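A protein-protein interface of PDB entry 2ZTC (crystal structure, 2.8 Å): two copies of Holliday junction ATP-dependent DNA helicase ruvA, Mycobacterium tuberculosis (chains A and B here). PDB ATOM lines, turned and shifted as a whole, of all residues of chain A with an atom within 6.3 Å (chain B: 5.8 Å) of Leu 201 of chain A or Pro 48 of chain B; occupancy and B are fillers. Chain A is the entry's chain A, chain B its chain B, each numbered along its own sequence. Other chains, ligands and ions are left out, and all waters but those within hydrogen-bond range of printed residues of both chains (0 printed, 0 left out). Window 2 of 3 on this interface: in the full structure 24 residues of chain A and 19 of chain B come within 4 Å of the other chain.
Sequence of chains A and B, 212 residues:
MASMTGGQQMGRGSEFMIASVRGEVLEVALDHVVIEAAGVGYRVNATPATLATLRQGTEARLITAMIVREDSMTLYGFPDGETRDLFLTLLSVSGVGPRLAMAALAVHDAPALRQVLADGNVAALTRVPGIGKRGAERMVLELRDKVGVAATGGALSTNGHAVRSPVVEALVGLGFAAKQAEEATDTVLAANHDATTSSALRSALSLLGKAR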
ATOM      1  N   PRO A 166     -19.906 -18.586 -34.425  1.00  0.00           N
ATOM      2  CA  PRO A 166     -20.653 -17.969 -33.327  1.00  0.00           C
ATOM      3  C   PRO A 166     -19.773 -16.961 -32.637  1.00  0.00           C
ATOM      4  O   PRO A 166     -20.121 -15.801 -32.479  1.00  0.00           O
ATOM      5  CB  PRO A 166     -20.847 -19.133 -32.356  1.00  0.00           C
ATOM      6  CG  PRO A 166     -20.889 -20.298 -33.172  1.00  0.00           C
ATOM      7  CD  PRO A 166     -20.059 -20.048 -34.416  1.00  0.00           C
ATOM      8  N   VAL A 167     -18.604 -17.441 -32.233  1.00  0.00           N
ATOM      9  CA  VAL A 167     -17.665 -16.650 -31.475  1.00  0.00           C
ATOM     10  C   VAL A 167     -17.317 -15.352 -32.148  1.00  0.00           C
ATOM     11  O   VAL A 167     -17.370 -14.290 -31.519  1.00  0.00           O
ATOM     12  CB  VAL A 167     -16.358 -17.383 -31.291  1.00  0.00           C
ATOM     13  CG1 VAL A 167     -15.358 -16.436 -30.689  1.00  0.00           C
ATOM     14  CG2 VAL A 167     -16.551 -18.600 -30.403  1.00  0.00           C
ATOM     15  N   ALA A 170     -20.086 -12.780 -32.207  1.00  0.00           N
ATOM     16  CA  ALA A 170     -20.143 -12.045 -30.945  1.00  0.00           C
ATOM     17  C   ALA A 170     -19.223 -10.835 -30.916  1.00  0.00           C
ATOM     18  O   ALA A 170     -19.649  -9.733 -30.571  1.00  0.00           O
ATOM     19  CB  ALA A 170     -19.817 -12.969 -29.775  1.00  0.00           C
ATOM     20  N   LEU A 171     -17.961 -11.045 -31.253  1.00  0.00           N
ATOM     21  CA  LEU A 171     -16.989  -9.964 -31.194  1.00  0.00           C
ATOM     22  C   LEU A 171     -17.442  -8.865 -32.120  1.00  0.00           C
ATOM     23  O   LEU A 171     -17.499  -7.698 -31.740  1.00  0.00           O
ATOM     24  CB  LEU A 171     -15.595 -10.440 -31.605  1.00  0.00           C
ATOM     25  CG  LEU A 171     -15.028 -11.647 -30.856  1.00  0.00           C
ATOM     26  CD1 LEU A 171     -13.756 -12.161 -31.531  1.00  0.00           C
ATOM     27  CD2 LEU A 171     -14.758 -11.286 -29.399  1.00  0.00           C
ATOM     28  N   LEU A 174     -19.517  -6.738 -30.514  1.00  0.00           N
ATOM     29  CA  LEU A 174     -18.878  -5.861 -29.544  1.00  0.00           C
ATOM     30  C   LEU A 174     -18.092  -4.761 -30.269  1.00  0.00           C
ATOM     31  O   LEU A 174     -17.356  -4.003 -29.652  1.00  0.00           O
ATOM     32  CB  LEU A 174     -18.002  -6.665 -28.574  1.00  0.00           C
ATOM     33  CG  LEU A 174     -18.672  -7.659 -27.600  1.00  0.00           C
ATOM     34  CD1 LEU A 174     -17.714  -8.763 -27.104  1.00  0.00           C
ATOM     35  CD2 LEU A 174     -19.288  -6.956 -26.394  1.00  0.00           C
ATOM     36  N   VAL A 188      -6.841 -18.330 -30.877  1.00  0.00           N
ATOM     37  CA  VAL A 188      -7.275 -18.925 -29.641  1.00  0.00           C
ATOM     38  C   VAL A 188      -7.513 -20.430 -29.839  1.00  0.00           C
ATOM     39  O   VAL A 188      -6.888 -21.244 -29.159  1.00  0.00           O
ATOM     40  CB  VAL A 188      -8.526 -18.152 -29.147  1.00  0.00           C
ATOM     41  CG1 VAL A 188      -9.129 -18.751 -27.869  1.00  0.00           C
ATOM     42  CG2 VAL A 188      -8.145 -16.704 -28.950  1.00  0.00           C
ATOM     43  N   THR A 196     -14.810 -24.323 -25.977  1.00  0.00           N
ATOM     44  CA  THR A 196     -16.246 -24.114 -26.196  1.00  0.00           C
ATOM     45  C   THR A 196     -16.554 -22.758 -26.780  1.00  0.00           C
ATOM     46  O   THR A 196     -15.685 -21.895 -26.884  1.00  0.00           O
ATOM     47  CB  THR A 196     -17.049 -24.194 -24.887  1.00  0.00           C
ATOM     48  OG1 THR A 196     -16.547 -23.226 -23.955  1.00  0.00           O
ATOM     49  CG2 THR A 196     -16.955 -25.563 -24.276  1.00  0.00           C
ATOM     50  N   THR A 197     -17.810 -22.560 -27.134  1.00  0.00           N
ATOM     51  CA  THR A 197     -18.176 -21.373 -27.869  1.00  0.00           C
ATOM     52  C   THR A 197     -18.000 -20.122 -27.015  1.00  0.00           C
ATOM     53  O   THR A 197     -17.785 -19.036 -27.524  1.00  0.00           O
ATOM     54  CB  THR A 197     -19.600 -21.490 -28.386  1.00  0.00           C
ATOM     55  OG1 THR A 197     -19.974 -20.254 -29.000  1.00  0.00           O
ATOM     56  CG2 THR A 197     -20.541 -21.817 -27.244  1.00  0.00           C
ATOM     57  N   SER A 198     -18.057 -20.292 -25.707  1.00  0.00           N
ATOM     58  CA  SER A 198     -17.906 -19.181 -24.783  1.00  0.00           C
ATOM     59  C   SER A 198     -16.500 -19.073 -24.199  1.00  0.00           C
ATOM     60  O   SER A 198     -15.935 -17.983 -24.102  1.00  0.00           O
ATOM     61  CB  SER A 198     -18.917 -19.325 -23.650  1.00  0.00           C
ATOM     62  OG  SER A 198     -18.544 -20.381 -22.785  1.00  0.00           O
ATOM     63  N   SER A 199     -15.932 -20.205 -23.797  1.00  0.00           N
ATOM     64  CA  SER A 199     -14.593 -20.181 -23.218  1.00  0.00           C
ATOM     65  C   SER A 199     -13.580 -19.646 -24.237  1.00  0.00           C
ATOM     66  O   SER A 199     -12.532 -19.100 -23.866  1.00  0.00           O
ATOM     67  CB  SER A 199     -14.206 -21.543 -22.615  1.00  0.00           C
ATOM     68  OG  SER A 199     -14.012 -22.548 -23.591  1.00  0.00           O
ATOM     69  N   ALA A 200     -13.923 -19.778 -25.515  1.00  0.00           N
ATOM     70  CA  ALA A 200     -13.211 -19.118 -26.608  1.00  0.00           C
ATOM     71  C   ALA A 200     -13.417 -17.630 -26.503  1.00  0.00           C
ATOM     72  O   ALA A 200     -12.469 -16.842 -26.526  1.00  0.00           O
ATOM     73  CB  ALA A 200     -13.768 -19.577 -27.926  1.00  0.00           C
ATOM     74  N   LEU A 201     -14.687 -17.255 -26.426  1.00  0.00           N
ATOM     75  CA  LEU A 201     -15.062 -15.861 -26.454  1.00  0.00           C
ATOM     76  C   LEU A 201     -14.208 -15.052 -25.487  1.00  0.00           C
ATOM     77  O   LEU A 201     -13.613 -14.038 -25.870  1.00  0.00           O
ATOM     78  CB  LEU A 201     -16.534 -15.720 -26.105  1.00  0.00           C
ATOM     79  CG  LEU A 201     -17.241 -14.750 -27.037  1.00  0.00           C
ATOM     80  CD1 LEU A 201     -18.551 -14.361 -26.440  1.00  0.00           C
ATOM     81  CD2 LEU A 201     -16.359 -13.548 -27.231  1.00  0.00           C
ATOM     82  N   ARG A 202     -14.141 -15.515 -24.240  1.00  0.00           N
ATOM     83  CA  ARG A 202     -13.395 -14.818 -23.190  1.00  0.00           C
ATOM     84  C   ARG A 202     -11.920 -14.724 -23.535  1.00  0.00           C
ATOM     85  O   ARG A 202     -11.341 -13.636 -23.481  1.00  0.00           O
ATOM     86  CB  ARG A 202     -13.577 -15.522 -21.843  1.00  0.00           C
ATOM     87  CG  ARG A 202     -15.006 -16.015 -21.613  1.00  0.00           C
ATOM     88  CD  ARG A 202     -15.047 -17.092 -20.559  1.00  0.00           C
ATOM     89  NE  ARG A 202     -16.053 -18.112 -20.843  1.00  0.00           N
ATOM     90  CZ  ARG A 202     -16.132 -19.270 -20.195  1.00  0.00           C
ATOM     91  NH1 ARG A 202     -15.261 -19.543 -19.231  1.00  0.00           N
ATOM     92  NH2 ARG A 202     -17.072 -20.152 -20.506  1.00  0.00           N
ATOM     93  N   SER A 203     -11.329 -15.860 -23.908  1.00  0.00           N
ATOM     94  CA  SER A 203      -9.907 -15.914 -24.234  1.00  0.00           C
ATOM     95  C   SER A 203      -9.622 -14.987 -25.387  1.00  0.00           C
ATOM     96  O   SER A 203      -8.600 -14.314 -25.441  1.00  0.00           O
ATOM     97  CB  SER A 203      -9.481 -17.330 -24.606  1.00  0.00           C
ATOM     98  OG  SER A 203      -9.690 -18.212 -23.528  1.00  0.00           O
ATOM     99  N   ALA A 204     -10.548 -14.959 -26.322  1.00  0.00           N
ATOM    100  CA  ALA A 204     -10.410 -14.082 -27.452  1.00  0.00           C
ATOM    101  C   ALA A 204     -10.482 -12.619 -26.976  1.00  0.00           C
ATOM    102  O   ALA A 204      -9.849 -11.730 -27.543  1.00  0.00           O
ATOM    103  CB  ALA A 204     -11.482 -14.410 -28.470  1.00  0.00           C
ATOM    104  N   LEU A 205     -11.236 -12.370 -25.916  1.00  0.00           N
ATOM    105  CA  LEU A 205     -11.293 -11.018 -25.388  1.00  0.00           C
ATOM    106  C   LEU A 205     -10.037 -10.707 -24.555  1.00  0.00           C
ATOM    107  O   LEU A 205      -9.416  -9.652 -24.729  1.00  0.00           O
ATOM    108  CB  LEU A 205     -12.618 -10.769 -24.649  1.00  0.00           C
ATOM    109  CG  LEU A 205     -13.886 -10.827 -25.554  1.00  0.00           C
ATOM    110  CD1 LEU A 205     -15.149 -11.060 -24.758  1.00  0.00           C
ATOM    111  CD2 LEU A 205     -14.091  -9.601 -26.421  1.00  0.00           C
ATOM    112  N   SER A 206      -9.634 -11.643 -23.694  1.00  0.00           N
ATOM    113  CA  SER A 206      -8.321 -11.569 -23.034  1.00  0.00           C
ATOM    114  C   SER A 206      -7.277 -11.176 -24.057  1.00  0.00           C
ATOM    115  O   SER A 206      -6.576 -10.181 -23.909  1.00  0.00           O
ATOM    116  CB  SER A 206      -7.907 -12.922 -22.444  1.00  0.00           C
ATOM    117  OG  SER A 206      -8.355 -13.094 -21.117  1.00  0.00           O
ATOM    118  N   LEU B  30     -24.278 -15.554 -25.824  1.00  0.00           N
ATOM    119  CA  LEU B  30     -22.944 -14.967 -25.822  1.00  0.00           C
ATOM    120  C   LEU B  30     -22.989 -13.491 -25.390  1.00  0.00           C
ATOM    121  O   LEU B  30     -21.967 -12.903 -25.070  1.00  0.00           O
ATOM    122  CB  LEU B  30     -22.343 -15.093 -27.228  1.00  0.00           C
ATOM    123  CG  LEU B  30     -22.023 -16.461 -27.856  1.00  0.00           C
ATOM    124  CD1 LEU B  30     -20.529 -16.694 -28.102  1.00  0.00           C
ATOM    125  CD2 LEU B  30     -22.642 -17.610 -27.041  1.00  0.00           C
ATOM    126  N   ALA B  46     -25.142  -8.976 -20.890  1.00  0.00           N
ATOM    127  CA  ALA B  46     -24.051  -9.243 -19.973  1.00  0.00           C
ATOM    128  C   ALA B  46     -22.748  -9.559 -20.714  1.00  0.00           C
ATOM    129  O   ALA B  46     -22.762  -9.957 -21.883  1.00  0.00           O
ATOM    130  CB  ALA B  46     -24.440 -10.386 -19.037  1.00  0.00           C
ATOM    131  N   THR B  47     -21.619  -9.367 -20.036  1.00  0.00           N
ATOM    132  CA  THR B  47     -20.351  -9.750 -20.619  1.00  0.00           C
ATOM    133  C   THR B  47     -20.192 -11.267 -20.582  1.00  0.00           C
ATOM    134  O   THR B  47     -20.727 -11.949 -19.708  1.00  0.00           O
ATOM    135  CB  THR B  47     -19.185  -9.107 -19.894  1.00  0.00           C
ATOM    136  OG1 THR B  47     -19.075  -9.682 -18.586  1.00  0.00           O
ATOM    137  CG2 THR B  47     -19.387  -7.601 -19.810  1.00  0.00           C
ATOM    138  N   PRO B  48     -19.451 -11.802 -21.547  1.00  0.00           N
ATOM    139  CA  PRO B  48     -19.187 -13.240 -21.583  1.00  0.00           C
ATOM    140  C   PRO B  48     -18.596 -13.639 -20.239  1.00  0.00           C
ATOM    141  O   PRO B  48     -18.958 -14.673 -19.670  1.00  0.00           O
ATOM    142  CB  PRO B  48     -18.152 -13.371 -22.699  1.00  0.00           C
ATOM    143  CG  PRO B  48     -18.384 -12.154 -23.572  1.00  0.00           C
ATOM    144  CD  PRO B  48     -18.776 -11.070 -22.634  1.00  0.00           C
ATOM    145  N   ALA B  49     -17.690 -12.799 -19.739  1.00  0.00           N
ATOM    146  CA  ALA B  49     -17.100 -12.985 -18.422  1.00  0.00           C
ATOM    147  C   ALA B  49     -18.185 -13.290 -17.387  1.00  0.00           C
ATOM    148  O   ALA B  49     -18.074 -14.249 -16.620  1.00  0.00           O
ATOM    149  CB  ALA B  49     -16.332 -11.751 -18.031  1.00  0.00           C
ATOM    150  N   THR B  50     -19.221 -12.450 -17.363  1.00  0.00           N
ATOM    151  CA  THR B  50     -20.372 -12.684 -16.497  1.00  0.00           C
ATOM    152  C   THR B  50     -21.130 -13.946 -16.906  1.00  0.00           C
ATOM    153  O   THR B  50     -21.337 -14.834 -16.078  1.00  0.00           O
ATOM    154  CB  THR B  50     -21.371 -11.512 -16.493  1.00  0.00           C
ATOM    155  OG1 THR B  50     -20.709 -10.292 -16.145  1.00  0.00           O
ATOM    156  CG2 THR B  50     -22.478 -11.785 -15.501  1.00  0.00           C
ATOM    157  N   LEU B  51     -21.568 -14.017 -18.167  1.00  0.00           N
ATOM    158  CA  LEU B  51     -22.339 -15.174 -18.630  1.00  0.00           C
ATOM    159  C   LEU B  51     -21.601 -16.464 -18.277  1.00  0.00           C
ATOM    160  O   LEU B  51     -22.225 -17.504 -18.064  1.00  0.00           O
ATOM    161  CB  LEU B  51     -22.546 -15.145 -20.145  1.00  0.00           C
ATOM    162  CG  LEU B  51     -23.174 -13.998 -20.924  1.00  0.00           C
ATOM    163  CD1 LEU B  51     -22.662 -13.981 -22.353  1.00  0.00           C
ATOM    164  CD2 LEU B  51     -24.685 -14.043 -20.863  1.00  0.00           C
ATOM    165  N   ALA B  52     -20.272 -16.369 -18.217  1.00  0.00           N
ATOM    166  CA  ALA B  52     -19.405 -17.528 -18.065  1.00  0.00           C
ATOM    167  C   ALA B  52     -19.809 -18.364 -16.865  1.00  0.00           C
ATOM    168  O   ALA B  52     -19.874 -19.587 -16.917  1.00  0.00           O
ATOM    169  CB  ALA B  52     -17.966 -17.085 -17.923  1.00  0.00           C
ATOM    170  N   THR B  53     -20.085 -17.682 -15.773  1.00  0.00           N
ATOM    171  CA  THR B  53     -20.376 -18.354 -14.526  1.00  0.00           C
ATOM    172  C   THR B  53     -21.758 -19.005 -14.564  1.00  0.00           C
ATOM    173  O   THR B  53     -22.078 -19.844 -13.722  1.00  0.00           O
ATOM    174  CB  THR B  53     -20.322 -17.358 -13.365  1.00  0.00           C
ATOM    175  OG1 THR B  53     -21.627 -17.213 -12.802  1.00  0.00           O
ATOM    176  CG2 THR B  53     -19.806 -15.989 -13.862  1.00  0.00           C
ATOM    177  N   ALA B 106     -16.591  -6.033 -21.335  1.00  0.00           N
ATOM    178  CA  ALA B 106     -16.556  -7.345 -21.916  1.00  0.00           C
ATOM    179  C   ALA B 106     -15.096  -7.667 -22.130  1.00  0.00           C
ATOM    180  O   ALA B 106     -14.647  -8.804 -21.924  1.00  0.00           O
ATOM    181  CB  ALA B 106     -17.318  -7.344 -23.229  1.00  0.00           C
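OG of Ser 198 of chain A lies within hydrogen-bond range of NH2 of Arg 202 of chain A (2.7 Å).
Among the printed residues, merely in contact across the chains: Leu 201 of chain A with Leu 30 of chain B (3.5 Å), Leu 205 of chain A with Pro 48 of chain B (3.6 Å), Leu 201 of chain A with Pro 48 of chain B (3.6 Å), Arg 202 of chain A with Ala 52 of chain B (3.6 Å), Thr 197 of chain A with Leu 30 of chain B (3.7 Å), Leu 205 of chain A with Ala 106 of chain B (3.7 Å) and Leu 174 of chain A with Ala 106 of chain B (3.7 Å).
Val 167 of chain A touches none of the printed residues of chain B. Printed residues of chain B within 4 Å of Thr 197 of chain A: Leu 30. Of chain B, only Leu 30 and Pro 48 come within 4 Å of Leu 201 of chain A. Printed residues of chain B within 4 Å of Arg 202 of chain A: Ala 52. Printed residues of chain A within 4 Å of Leu 30 of chain B: Thr 197 (3.7 Å) and Leu 201 (3.5 Å). Of chain A, only Leu 201 (3.6 Å) and Leu 205 (3.6 Å) come within 4 Å of Pro 48 of chain B. Of the printed residues of chain A, Ala 52 of chain B touches Arg 202 (3.6 Å).
Along chain A the printed residues that touch a printed residue of chain B span positions 174 to 205. Hydrophobic or aromatic side chains of chain B that line the printed part of chain A: Leu 30, Pro 48, Ala 52 and Ala 106. Among the printed residues, 7 pairs touch across the chains. Among the printed residues, no Asp or Glu carboxylate lies within 4 Å of a Lys or Arg side-chain nitrogen of the other chain.
No position is printed for both chains.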
